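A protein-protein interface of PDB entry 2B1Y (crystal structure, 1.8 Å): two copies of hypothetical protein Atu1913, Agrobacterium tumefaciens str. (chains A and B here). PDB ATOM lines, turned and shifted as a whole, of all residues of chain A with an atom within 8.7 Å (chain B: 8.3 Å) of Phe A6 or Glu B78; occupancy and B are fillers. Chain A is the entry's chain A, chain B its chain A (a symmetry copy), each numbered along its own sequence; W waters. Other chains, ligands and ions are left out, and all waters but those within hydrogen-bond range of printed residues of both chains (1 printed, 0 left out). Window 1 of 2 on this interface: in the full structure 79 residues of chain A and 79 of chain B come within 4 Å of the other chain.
Water W1 lies within hydrogen-bond range of the side-chain carboxylate of Glu B78 (2.5 Å) and the guanidinium group of Arg A33 (2.9 Å).
The backbone carbonyl oxygen (O) of Arg A33 sits at hydrogen-bond distance from the backbone NH (N) of Ile B74.
NE2 of His B80 is in hydrogen-bond range of OD1 of Asn A31, 2.7 Å away.
The backbone NH of Ala B77 sits at hydrogen-bond distance from the backbone carbonyl oxygen of Arg A7, at 3.1 Å.
The side-chain amide nitrogen (ND2) of Asn A30 lies close to the backbone carbonyl oxygen (O) of Asp B76 (3.4 Å).
O of Glu B78 lies within hydrogen-bond range of ND2 of Asn A31 (3.0 Å).
The side-chain amide nitrogen of Asn A31 is in hydrogen-bond range of the side-chain carboxylate of Asp B76.
The guanidinium group (NE) of Arg A33 lies within salt-bridge range of the side-chain carboxylate (OD1) of Asp B76 (2.6 Å).
The backbone carbonyl oxygen of Ile B75 lies within hydrogen-bond range of the backbone NH of Thr A9, at 2.7 Å.
NH1 of Arg A33 is in salt-bridge range of OE1 of Glu B78.
O of Gly B82 sits close to OD1 of Asn A30 (2.9 Å).
Positions printed for both chains: 49, 51 and 78.
Phe A6 touches just these residues of chain B: Asp B76 and Glu B78.
Printed residues of chain B within 4 Å of Val A32: Ile B74 and Ile B75.
Glu A45 touches none of the printed residues of chain B.
Leu A47 touches none of the printed residues of chain B.
Printed residues of chain A within 4 Å of Val B55: Val A29 (3.7 Å), Asn A30 (3.7 Å) and Asn A31 (3.6 Å).
Printed residues of chain A within 4 Å of Ile B75: Tyr A8, Thr A9, Asn A30, Asn A31 and Val A32.
Of chain A, only Arg A7 comes within 4 Å of Ala B77.
Glu B78 touches just these residues of chain A: Phe A6, Asn A31 and Arg A33.
CE2 of Phe A6 touches CB of Asp B76 (3.8 Å).
Glu B78 touches Phe A6 (CB to CD1, 3.9 Å).
Leu B83 touches Arg A7.
Tyr A8 touches Asp B76 (CB to CB, 3.5 Å).
Thr A9 touches Ile B74 (O to CA, 3.4 Å).
CA of Ile B75 touches O of Asn A31, 3.4 Å away.
CA of Val A32 touches O of Ile B74 (3.5 Å).
Val A32 touches Ile B75 (CG2 to CD1, 3.8 Å).
Met A35 touches Phe B49.
CG2 of Ile B74 touches CZ of Phe A43, 3.6 Å away.
Hydrophobic or aromatic side chains of chain B that line the printed part of chain A: Phe B49, Tyr B51, Val B55, Ile B74, Ile B75, Ala B77, His B80 and Leu B83.
Among the printed residues, 36 pairs touch across the chains.
Among the printed residues, Asp or Glu carboxylates within 4 Å of a Lys or Arg side-chain nitrogen of the other chain: Arg A33 with Asp B76 (2.6 Å) and Arg A33 with Glu B78 (2.6 Å).
The backbone NH (N) of Glu B78 is in hydrogen-bond range of the side-chain carboxylate (OD2) of Asp B76, at 2.9 Å.
ND2 of Asn A5 sits at hydrogen-bond distance from O of Leu A46.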
ATOM      1  N   PRO A   4     -26.322   9.175  -7.222  1.00  0.00           N
ATOM      2  CA  PRO A   4     -26.220  10.126  -6.107  1.00  0.00           C
ATOM      3  C   PRO A   4     -25.938  11.532  -6.620  1.00  0.00           C
ATOM      4  O   PRO A   4     -25.139  11.703  -7.568  1.00  0.00           O
ATOM      5  CB  PRO A   4     -25.019   9.611  -5.302  1.00  0.00           C
ATOM      6  CG  PRO A   4     -24.806   8.193  -5.778  1.00  0.00           C
ATOM      7  CD  PRO A   4     -25.229   8.195  -7.216  1.00  0.00           C
ATOM      8  N   ASN A   5     -26.584  12.530  -6.023  1.00  0.00           N
ATOM      9  CA  ASN A   5     -26.470  13.888  -6.543  1.00  0.00           C
ATOM     10  C   ASN A   5     -25.035  14.443  -6.512  1.00  0.00           C
ATOM     11  O   ASN A   5     -24.660  15.251  -7.369  1.00  0.00           O
ATOM     12  CB  ASN A   5     -27.458  14.843  -5.854  1.00  0.00           C
ATOM     13  CG  ASN A   5     -28.913  14.668  -6.344  1.00  0.00           C
ATOM     14  OD1 ASN A   5     -29.165  14.199  -7.451  1.00  0.00           O
ATOM     15  ND2 ASN A   5     -29.869  15.059  -5.506  1.00  0.00           N
ATOM     16  N   PHE A   6     -24.230  13.998  -5.545  1.00  0.00           N
ATOM     17  CA  PHE A   6     -22.838  14.496  -5.380  1.00  0.00           C
ATOM     18  C   PHE A   6     -22.089  13.540  -4.454  1.00  0.00           C
ATOM     19  O   PHE A   6     -22.721  12.742  -3.761  1.00  0.00           O
ATOM     20  CB  PHE A   6     -22.838  15.901  -4.784  1.00  0.00           C
ATOM     21  CG  PHE A   6     -23.660  16.026  -3.520  1.00  0.00           C
ATOM     22  CD1 PHE A   6     -24.984  16.451  -3.584  1.00  0.00           C
ATOM     23  CD2 PHE A   6     -23.115  15.684  -2.262  1.00  0.00           C
ATOM     24  CE1 PHE A   6     -25.761  16.557  -2.400  1.00  0.00           C
ATOM     25  CE2 PHE A   6     -23.886  15.790  -1.093  1.00  0.00           C
ATOM     26  CZ  PHE A   6     -25.207  16.220  -1.168  1.00  0.00           C
ATOM     27  N   ARG A   7     -20.757  13.617  -4.424  1.00  0.00           N
ATOM     28  CA  ARG A   7     -19.969  12.709  -3.617  1.00  0.00           C
ATOM     29  C   ARG A   7     -19.839  13.263  -2.199  1.00  0.00           C
ATOM     30  O   ARG A   7     -19.917  14.462  -1.986  1.00  0.00           O
ATOM     31  CB  ARG A   7     -18.572  12.467  -4.224  1.00  0.00           C
ATOM     32  CG  ARG A   7     -18.568  11.730  -5.609  1.00  0.00           C
ATOM     33  CD  ARG A   7     -17.167  11.322  -6.004  1.00  0.00           C
ATOM     34  NE  ARG A   7     -16.698  10.337  -5.046  1.00  0.00           N
ATOM     35  CZ  ARG A   7     -15.461  10.249  -4.585  1.00  0.00           C
ATOM     36  NH1 ARG A   7     -15.187   9.324  -3.695  1.00  0.00           N
ATOM     37  NH2 ARG A   7     -14.522  11.079  -5.008  1.00  0.00           N
ATOM     38  N   TYR A   8     -19.626  12.387  -1.246  1.00  0.00           N
ATOM     39  CA  TYR A   8     -19.465  12.837   0.147  1.00  0.00           C
ATOM     40  C   TYR A   8     -18.694  11.800   0.945  1.00  0.00           C
ATOM     41  O   TYR A   8     -18.569  10.631   0.535  1.00  0.00           O
ATOM     42  CB  TYR A   8     -20.836  13.105   0.814  1.00  0.00           C
ATOM     43  CG  TYR A   8     -21.621  11.847   1.085  1.00  0.00           C
ATOM     44  CD1 TYR A   8     -22.345  11.239   0.062  1.00  0.00           C
ATOM     45  CD2 TYR A   8     -21.621  11.251   2.348  1.00  0.00           C
ATOM     46  CE1 TYR A   8     -23.052  10.067   0.292  1.00  0.00           C
ATOM     47  CE2 TYR A   8     -22.318  10.076   2.589  1.00  0.00           C
ATOM     48  CZ  TYR A   8     -23.038   9.497   1.538  1.00  0.00           C
ATOM     49  OH  TYR A   8     -23.759   8.348   1.741  1.00  0.00           O
ATOM     50  N   THR A   9     -18.206  12.228   2.112  1.00  0.00           N
ATOM     51  CA  THR A   9     -17.569  11.340   3.042  1.00  0.00           C
ATOM     52  C   THR A   9     -18.300  11.457   4.370  1.00  0.00           C
ATOM     53  O   THR A   9     -18.566  12.557   4.813  1.00  0.00           O
ATOM     54  CB  THR A   9     -16.133  11.812   3.316  1.00  0.00           C
ATOM     55  OG1 THR A   9     -15.380  11.756   2.104  1.00  0.00           O
ATOM     56  CG2 THR A   9     -15.491  10.920   4.377  1.00  0.00           C
ATOM     57  N   VAL A  29     -11.521  23.349  -1.298  1.00  0.00           N
ATOM     58  CA  VAL A  29     -12.864  23.896  -0.936  1.00  0.00           C
ATOM     59  C   VAL A  29     -13.962  22.820  -1.035  1.00  0.00           C
ATOM     60  O   VAL A  29     -14.135  22.192  -2.080  1.00  0.00           O
ATOM     61  CB  VAL A  29     -13.192  25.123  -1.832  1.00  0.00           C
ATOM     62  CG1 VAL A  29     -14.583  25.732  -1.505  1.00  0.00           C
ATOM     63  CG2 VAL A  29     -12.121  26.155  -1.641  1.00  0.00           C
ATOM     64  N   ASN A  30     -14.651  22.580   0.086  1.00  0.00           N
ATOM     65  CA  ASN A  30     -15.774  21.649   0.170  1.00  0.00           C
ATOM     66  C   ASN A  30     -16.677  22.075   1.315  1.00  0.00           C
ATOM     67  O   ASN A  30     -16.352  23.008   2.060  1.00  0.00           O
ATOM     68  CB  ASN A  30     -15.305  20.205   0.416  1.00  0.00           C
ATOM     69  CG  ASN A  30     -15.330  19.343  -0.829  1.00  0.00           C
ATOM     70  OD1 ASN A  30     -15.258  19.824  -1.978  1.00  0.00           O
ATOM     71  ND2 ASN A  30     -15.398  18.046  -0.612  1.00  0.00           N
ATOM     72  N   ASN A  31     -17.814  21.401   1.441  1.00  0.00           N
ATOM     73  CA  ASN A  31     -18.749  21.704   2.527  1.00  0.00           C
ATOM     74  C   ASN A  31     -18.447  20.805   3.707  1.00  0.00           C
ATOM     75  O   ASN A  31     -18.078  19.642   3.531  1.00  0.00           O
ATOM     76  CB  ASN A  31     -20.195  21.424   2.090  1.00  0.00           C
ATOM     77  CG  ASN A  31     -20.549  22.161   0.806  1.00  0.00           C
ATOM     78  OD1 ASN A  31     -20.240  23.340   0.665  1.00  0.00           O
ATOM     79  ND2 ASN A  31     -21.151  21.463  -0.125  1.00  0.00           N
ATOM     80  N   VAL A  32     -18.649  21.348   4.896  1.00  0.00           N
ATOM     81  CA  VAL A  32     -18.450  20.582   6.112  1.00  0.00           C
ATOM     82  C   VAL A  32     -19.724  20.733   6.917  1.00  0.00           C
ATOM     83  O   VAL A  32     -20.143  21.851   7.185  1.00  0.00           O
ATOM     84  CB  VAL A  32     -17.236  21.149   6.911  1.00  0.00           C
ATOM     85  CG1 VAL A  32     -17.080  20.456   8.313  1.00  0.00           C
ATOM     86  CG2 VAL A  32     -15.979  20.987   6.119  1.00  0.00           C
ATOM     87  N   ARG A  33     -20.336  19.623   7.313  1.00  0.00           N
ATOM     88  CA  ARG A  33     -21.639  19.705   7.989  1.00  0.00           C
ATOM     89  C   ARG A  33     -21.611  18.722   9.146  1.00  0.00           C
ATOM     90  O   ARG A  33     -21.424  17.522   8.927  1.00  0.00           O
ATOM     91  CB  ARG A  33     -22.766  19.292   7.038  1.00  0.00           C
ATOM     92  CG  ARG A  33     -22.662  19.798   5.620  1.00  0.00           C
ATOM     93  CD  ARG A  33     -23.958  19.494   4.867  1.00  0.00           C
ATOM     94  NE  ARG A  33     -23.761  19.471   3.425  1.00  0.00           N
ATOM     95  CZ  ARG A  33     -24.668  19.823   2.520  1.00  0.00           C
ATOM     96  NH1 ARG A  33     -24.355  19.722   1.228  1.00  0.00           N
ATOM     97  NH2 ARG A  33     -25.860  20.294   2.892  1.00  0.00           N
ATOM     98  N   MET A  35     -23.950  17.103  12.063  1.00  0.00           N
ATOM     99  CA  MET A  35     -25.393  16.916  12.254  1.00  0.00           C
ATOM    100  C   MET A  35     -25.723  15.760  13.166  1.00  0.00           C
ATOM    101  O   MET A  35     -24.910  14.857  13.380  1.00  0.00           O
ATOM    102  CB  MET A  35     -26.058  16.690  10.881  1.00  0.00           C
ATOM    103  CG  MET A  35     -25.460  15.469  10.143  1.00  0.00           C
ATOM    104  SD  MET A  35     -26.165  15.276   8.331  1.00  0.00           S
ATOM    105  CE  MET A  35     -25.058  16.573   7.448  1.00  0.00           C
ATOM    106  N   PHE A  43     -30.294  13.889   5.405  1.00  0.00           N
ATOM    107  CA  PHE A  43     -29.240  14.016   4.411  1.00  0.00           C
ATOM    108  C   PHE A  43     -29.240  12.851   3.386  1.00  0.00           C
ATOM    109  O   PHE A  43     -29.159  13.080   2.174  1.00  0.00           O
ATOM    110  CB  PHE A  43     -27.870  14.095   5.104  1.00  0.00           C
ATOM    111  CG  PHE A  43     -26.708  14.179   4.155  1.00  0.00           C
ATOM    112  CD1 PHE A  43     -26.341  15.408   3.593  1.00  0.00           C
ATOM    113  CD2 PHE A  43     -25.960  13.041   3.849  1.00  0.00           C
ATOM    114  CE1 PHE A  43     -25.262  15.494   2.713  1.00  0.00           C
ATOM    115  CE2 PHE A  43     -24.889  13.140   2.979  1.00  0.00           C
ATOM    116  CZ  PHE A  43     -24.533  14.377   2.442  1.00  0.00           C
ATOM    117  N   THR A  44     -29.337  11.618   3.866  1.00  0.00           N
ATOM    118  CA  THR A  44     -29.270  10.465   2.958  1.00  0.00           C
ATOM    119  C   THR A  44     -30.458  10.457   1.995  1.00  0.00           C
ATOM    120  O   THR A  44     -30.336   9.971   0.871  1.00  0.00           O
ATOM    121  CB  THR A  44     -29.187   9.111   3.685  1.00  0.00           C
ATOM    122  OG1 THR A  44     -30.436   8.831   4.330  1.00  0.00           O
ATOM    123  CG2 THR A  44     -28.035   9.107   4.699  1.00  0.00           C
ATOM    124  N   GLU A  45     -31.591  11.012   2.436  1.00  0.00           N
ATOM    125  CA  GLU A  45     -32.753  11.185   1.560  1.00  0.00           C
ATOM    126  C   GLU A  45     -32.471  12.205   0.482  1.00  0.00           C
ATOM    127  O   GLU A  45     -32.830  11.983  -0.670  1.00  0.00           O
ATOM    128  CB  GLU A  45     -34.032  11.519   2.358  1.00  0.00           C
ATOM    129  CG  GLU A  45     -34.394  10.494   3.450  1.00  0.00           C
ATOM    130  CD  GLU A  45     -34.632   9.085   2.922  1.00  0.00           C
ATOM    131  OE1 GLU A  45     -35.631   8.887   2.201  1.00  0.00           O
ATOM    132  OE2 GLU A  45     -33.826   8.172   3.220  1.00  0.00           O
ATOM    133  N   LEU A  46     -31.785  13.280   0.822  1.00  0.00           N
ATOM    134  CA  LEU A  46     -31.546  14.328  -0.143  1.00  0.00           C
ATOM    135  C   LEU A  46     -30.446  14.011  -1.189  1.00  0.00           C
ATOM    136  O   LEU A  46     -30.334  14.692  -2.215  1.00  0.00           O
ATOM    137  CB  LEU A  46     -31.380  15.664   0.598  1.00  0.00           C
ATOM    138  CG  LEU A  46     -32.572  15.918   1.558  1.00  0.00           C
ATOM    139  CD1 LEU A  46     -32.249  16.974   2.619  1.00  0.00           C
ATOM    140  CD2 LEU A  46     -33.878  16.261   0.837  1.00  0.00           C
ATOM    141  N   LEU A  47     -29.677  12.940  -0.962  1.00  0.00           N
ATOM    142  CA  LEU A  47     -28.760  12.432  -1.987  1.00  0.00           C
ATOM    143  C   LEU A  47     -29.504  11.856  -3.200  1.00  0.00           C
ATOM    144  O   LEU A  47     -28.950  11.823  -4.293  1.00  0.00           O
ATOM    145  CB  LEU A  47     -27.822  11.381  -1.409  1.00  0.00           C
ATOM    146  CG  LEU A  47     -26.653  11.857  -0.546  1.00  0.00           C
ATOM    147  CD1 LEU A  47     -26.228  10.672   0.288  1.00  0.00           C
ATOM    148  CD2 LEU A  47     -25.526  12.284  -1.431  1.00  0.00           C
ATOM    149  N   ASP A  48     -30.746  11.417  -3.000  1.00  0.00           N
ATOM    150  CA  ASP A  48     -31.560  10.867  -4.095  1.00  0.00           C
ATOM    151  C   ASP A  48     -32.721  11.796  -4.523  1.00  0.00           C
ATOM    152  O   ASP A  48     -33.598  11.382  -5.314  1.00  0.00           O
ATOM    153  CB  ASP A  48     -32.134   9.483  -3.717  1.00  0.00           C
ATOM    154  CG  ASP A  48     -31.058   8.436  -3.513  1.00  0.00           C
ATOM    155  OD1 ASP A  48     -29.975   8.546  -4.142  1.00  0.00           O
ATOM    156  OD2 ASP A  48     -31.296   7.510  -2.708  1.00  0.00           O
ATOM    157  N   PHE A  49     -32.733  13.026  -4.011  1.00  0.00           N
ATOM    158  CA  PHE A  49     -33.837  13.957  -4.295  1.00  0.00           C
ATOM    159  C   PHE A  49     -33.734  14.513  -5.715  1.00  0.00           C
ATOM    160  O   PHE A  49     -32.715  15.130  -6.099  1.00  0.00           O
ATOM    161  CB  PHE A  49     -33.858  15.080  -3.251  1.00  0.00           C
ATOM    162  CG  PHE A  49     -34.910  16.116  -3.496  1.00  0.00           C
ATOM    163  CD1 PHE A  49     -36.237  15.748  -3.810  1.00  0.00           C
ATOM    164  CD2 PHE A  49     -34.589  17.478  -3.338  1.00  0.00           C
ATOM    165  CE1 PHE A  49     -37.231  16.739  -4.011  1.00  0.00           C
ATOM    166  CE2 PHE A  49     -35.568  18.465  -3.531  1.00  0.00           C
ATOM    167  CZ  PHE A  49     -36.876  18.099  -3.877  1.00  0.00           C
ATOM    168  N   LYS A  50     -34.765  14.244  -6.516  1.00  0.00           N
ATOM    169  CA  LYS A  50     -34.785  14.655  -7.926  1.00  0.00           C
ATOM    170  C   LYS A  50     -36.100  15.367  -8.231  1.00  0.00           C
ATOM    171  O   LYS A  50     -37.159  14.977  -7.706  1.00  0.00           O
ATOM    172  CB  LYS A  50     -34.705  13.432  -8.854  1.00  0.00           C
ATOM    173  CG  LYS A  50     -33.461  12.520  -8.656  1.00  0.00           C
ATOM    174  CD  LYS A  50     -32.200  13.178  -9.192  1.00  0.00           C
ATOM    175  CE  LYS A  50     -31.033  12.187  -9.130  1.00  0.00           C
ATOM    176  NZ  LYS A  50     -29.826  12.886  -9.689  1.00  0.00           N
ATOM    177  N   TYR A  51     -36.034  16.394  -9.086  1.00  0.00           N
ATOM    178  CA  TYR A  51     -37.245  17.074  -9.525  1.00  0.00           C
ATOM    179  C   TYR A  51     -36.970  17.803 -10.830  1.00  0.00           C
ATOM    180  O   TYR A  51     -35.811  17.957 -11.259  1.00  0.00           O
ATOM    181  CB  TYR A  51     -37.787  18.068  -8.450  1.00  0.00           C
ATOM    182  CG  TYR A  51     -36.788  19.172  -8.166  1.00  0.00           C
ATOM    183  CD1 TYR A  51     -35.807  19.019  -7.182  1.00  0.00           C
ATOM    184  CD2 TYR A  51     -36.804  20.359  -8.906  1.00  0.00           C
ATOM    185  CE1 TYR A  51     -34.864  20.048  -6.929  1.00  0.00           C
ATOM    186  CE2 TYR A  51     -35.881  21.363  -8.675  1.00  0.00           C
ATOM    187  CZ  TYR A  51     -34.922  21.204  -7.684  1.00  0.00           C
ATOM    188  OH  TYR A  51     -34.026  22.222  -7.481  1.00  0.00           O
ATOM    189  N   GLU A  78     -37.413  28.779  -1.243  1.00  0.00           N
ATOM    190  CA  GLU A  78     -36.015  28.507  -0.879  1.00  0.00           C
ATOM    191  C   GLU A  78     -35.026  29.477  -1.561  1.00  0.00           C
ATOM    192  O   GLU A  78     -34.974  29.541  -2.767  1.00  0.00           O
ATOM    193  CB  GLU A  78     -35.639  27.053  -1.180  1.00  0.00           C
ATOM    194  CG  GLU A  78     -34.196  26.764  -0.761  1.00  0.00           C
ATOM    195  CD  GLU A  78     -33.769  25.307  -0.918  1.00  0.00           C
ATOM    196  OE1 GLU A  78     -34.276  24.595  -1.809  1.00  0.00           O
ATOM    197  OE2 GLU A  78     -32.883  24.886  -0.134  1.00  0.00           O
ATOM    198  N   PHE B  49     -34.372  19.694   7.601  1.00  0.00           N
ATOM    199  CA  PHE B  49     -32.940  19.352   7.594  1.00  0.00           C
ATOM    200  C   PHE B  49     -32.101  20.490   8.175  1.00  0.00           C
ATOM    201  O   PHE B  49     -32.137  21.640   7.682  1.00  0.00           O
ATOM    202  CB  PHE B  49     -32.495  18.992   6.172  1.00  0.00           C
ATOM    203  CG  PHE B  49     -31.033  18.692   6.052  1.00  0.00           C
ATOM    204  CD1 PHE B  49     -30.386  17.838   6.971  1.00  0.00           C
ATOM    205  CD2 PHE B  49     -30.309  19.210   4.961  1.00  0.00           C
ATOM    206  CE1 PHE B  49     -29.008  17.538   6.830  1.00  0.00           C
ATOM    207  CE2 PHE B  49     -28.944  18.916   4.811  1.00  0.00           C
ATOM    208  CZ  PHE B  49     -28.296  18.095   5.745  1.00  0.00           C
ATOM    209  N   TYR B  51     -28.176  21.531  10.096  1.00  0.00           N
ATOM    210  CA  TYR B  51     -26.804  21.139  10.393  1.00  0.00           C
ATOM    211  C   TYR B  51     -25.986  22.377  10.723  1.00  0.00           C
ATOM    212  O   TYR B  51     -26.421  23.523  10.508  1.00  0.00           O
ATOM    213  CB  TYR B  51     -26.148  20.351   9.216  1.00  0.00           C
ATOM    214  CG  TYR B  51     -26.060  21.200   7.963  1.00  0.00           C
ATOM    215  CD1 TYR B  51     -27.109  21.231   7.040  1.00  0.00           C
ATOM    216  CD2 TYR B  51     -24.939  22.000   7.719  1.00  0.00           C
ATOM    217  CE1 TYR B  51     -27.031  22.038   5.877  1.00  0.00           C
ATOM    218  CE2 TYR B  51     -24.858  22.800   6.594  1.00  0.00           C
ATOM    219  CZ  TYR B  51     -25.901  22.809   5.677  1.00  0.00           C
ATOM    220  OH  TYR B  51     -25.784  23.612   4.571  1.00  0.00           O
ATOM    221  N   VAL B  55     -19.520  26.132   3.815  1.00  0.00           N
ATOM    222  CA  VAL B  55     -18.412  25.999   2.867  1.00  0.00           C
ATOM    223  C   VAL B  55     -17.101  26.298   3.569  1.00  0.00           C
ATOM    224  O   VAL B  55     -16.940  27.373   4.182  1.00  0.00           O
ATOM    225  CB  VAL B  55     -18.529  27.012   1.712  1.00  0.00           C
ATOM    226  CG1 VAL B  55     -17.413  26.745   0.699  1.00  0.00           C
ATOM    227  CG2 VAL B  55     -19.877  26.929   1.051  1.00  0.00           C
ATOM    228  N   ILE B  74     -20.217  15.251   7.882  1.00  0.00           N
ATOM    229  CA  ILE B  74     -20.222  15.049   6.438  1.00  0.00           C
ATOM    230  C   ILE B  74     -19.273  16.014   5.818  1.00  0.00           C
ATOM    231  O   ILE B  74     -19.343  17.202   6.100  1.00  0.00           O
ATOM    232  CB  ILE B  74     -21.633  15.286   5.839  1.00  0.00           C
ATOM    233  CG1 ILE B  74     -22.605  14.251   6.378  1.00  0.00           C
ATOM    234  CG2 ILE B  74     -21.592  15.330   4.284  1.00  0.00           C
ATOM    235  CD1 ILE B  74     -22.243  12.832   6.180  1.00  0.00           C
ATOM    236  N   ILE B  75     -18.405  15.505   4.952  1.00  0.00           N
ATOM    237  CA  ILE B  75     -17.639  16.345   4.028  1.00  0.00           C
ATOM    238  C   ILE B  75     -18.210  16.085   2.644  1.00  0.00           C
ATOM    239  O   ILE B  75     -18.334  14.930   2.244  1.00  0.00           O
ATOM    240  CB  ILE B  75     -16.132  15.953   4.011  1.00  0.00           C
ATOM    241  CG1 ILE B  75     -15.578  15.947   5.456  1.00  0.00           C
ATOM    242  CG2 ILE B  75     -15.349  16.879   3.082  1.00  0.00           C
ATOM    243  CD1 ILE B  75     -15.680  17.248   6.155  1.00  0.00           C
ATOM    244  N   ASP B  76     -18.573  17.132   1.911  1.00  0.00           N
ATOM    245  CA  ASP B  76     -19.240  16.847   0.637  1.00  0.00           C
ATOM    246  C   ASP B  76     -19.006  17.876  -0.442  1.00  0.00           C
ATOM    247  O   ASP B  76     -18.635  19.025  -0.187  1.00  0.00           O
ATOM    248  CB  ASP B  76     -20.748  16.643   0.852  1.00  0.00           C
ATOM    249  CG  ASP B  76     -21.474  17.957   1.146  1.00  0.00           C
ATOM    250  OD1 ASP B  76     -21.686  18.284   2.321  1.00  0.00           O
ATOM    251  OD2 ASP B  76     -21.761  18.702   0.192  1.00  0.00           O
ATOM    252  N   ALA B  77     -19.269  17.444  -1.669  1.00  0.00           N
ATOM    253  CA  ALA B  77     -18.964  18.235  -2.836  1.00  0.00           C
ATOM    254  C   ALA B  77     -20.197  18.903  -3.444  1.00  0.00           C
ATOM    255  O   ALA B  77     -20.166  19.278  -4.617  1.00  0.00           O
ATOM    256  CB  ALA B  77     -18.264  17.367  -3.873  1.00  0.00           C
ATOM    257  N   GLU B  78     -21.267  19.088  -2.675  1.00  0.00           N
ATOM    258  CA  GLU B  78     -22.432  19.778  -3.246  1.00  0.00           C
ATOM    259  C   GLU B  78     -22.091  21.198  -3.748  1.00  0.00           C
ATOM    260  O   GLU B  78     -21.649  22.023  -2.982  1.00  0.00           O
ATOM    261  CB  GLU B  78     -23.592  19.823  -2.246  1.00  0.00           C
ATOM    262  CG  GLU B  78     -24.815  20.505  -2.860  1.00  0.00           C
ATOM    263  CD  GLU B  78     -26.059  20.495  -1.976  1.00  0.00           C
ATOM    264  OE1 GLU B  78     -25.948  20.496  -0.733  1.00  0.00           O
ATOM    265  OE2 GLU B  78     -27.172  20.508  -2.557  1.00  0.00           O
ATOM    266  N   GLY B  79     -22.286  21.484  -5.036  1.00  0.00           N
ATOM    267  CA  GLY B  79     -21.914  22.782  -5.579  1.00  0.00           C
ATOM    268  C   GLY B  79     -20.435  22.994  -5.866  1.00  0.00           C
ATOM    269  O   GLY B  79     -20.015  24.117  -6.189  1.00  0.00           O
ATOM    270  N   HIS B  80     -19.638  21.925  -5.755  1.00  0.00           N
ATOM    271  CA  HIS B  80     -18.189  22.004  -5.912  1.00  0.00           C
ATOM    272  C   HIS B  80     -17.768  20.986  -6.995  1.00  0.00           C
ATOM    273  O   HIS B  80     -18.517  20.078  -7.325  1.00  0.00           O
ATOM    274  CB  HIS B  80     -17.487  21.737  -4.554  1.00  0.00           C
ATOM    275  CG  HIS B  80     -17.953  22.632  -3.439  1.00  0.00           C
ATOM    276  ND1 HIS B  80     -17.846  24.007  -3.486  1.00  0.00           N
ATOM    277  CD2 HIS B  80     -18.537  22.344  -2.250  1.00  0.00           C
ATOM    278  CE1 HIS B  80     -18.351  24.530  -2.382  1.00  0.00           C
ATOM    279  NE2 HIS B  80     -18.769  23.539  -1.607  1.00  0.00           N
ATOM    280  N   SER B  81     -16.592  21.140  -7.571  1.00  0.00           N
ATOM    281  CA  SER B  81     -16.260  20.281  -8.725  1.00  0.00           C
ATOM    282  C   SER B  81     -15.977  18.844  -8.319  1.00  0.00           C
ATOM    283  O   SER B  81     -16.298  17.917  -9.077  1.00  0.00           O
ATOM    284  CB  SER B  81     -15.086  20.819  -9.492  1.00  0.00           C
ATOM    285  OG  SER B  81     -13.953  20.747  -8.661  1.00  0.00           O
ATOM    286  N   GLY B  82     -15.406  18.672  -7.118  1.00  0.00           N
ATOM    287  CA  GLY B  82     -14.980  17.354  -6.645  1.00  0.00           C
ATOM    288  C   GLY B  82     -14.918  17.229  -5.125  1.00  0.00           C
ATOM    289  O   GLY B  82     -15.064  18.224  -4.408  1.00  0.00           O
ATOM    290  N   LEU B  83     -14.708  15.994  -4.653  1.00  0.00           N
ATOM    291  CA  LEU B  83     -14.677  15.698  -3.217  1.00  0.00           C
ATOM    292  C   LEU B  83     -13.275  15.857  -2.634  1.00  0.00           C
ATOM    293  O   LEU B  83     -12.299  15.260  -3.125  1.00  0.00           O
ATOM    294  CB  LEU B  83     -15.222  14.275  -2.956  1.00  0.00           C
ATOM    295  CG  LEU B  83     -15.284  13.837  -1.479  1.00  0.00           C
ATOM    296  CD1 LEU B  83     -16.269  14.674  -0.652  1.00  0.00           C
ATOM    297  CD2 LEU B  83     -15.594  12.305  -1.362  1.00  0.00           C
HETATM  298  O   HOH W   1     -27.591  21.485   0.899  1.00  0.00           O
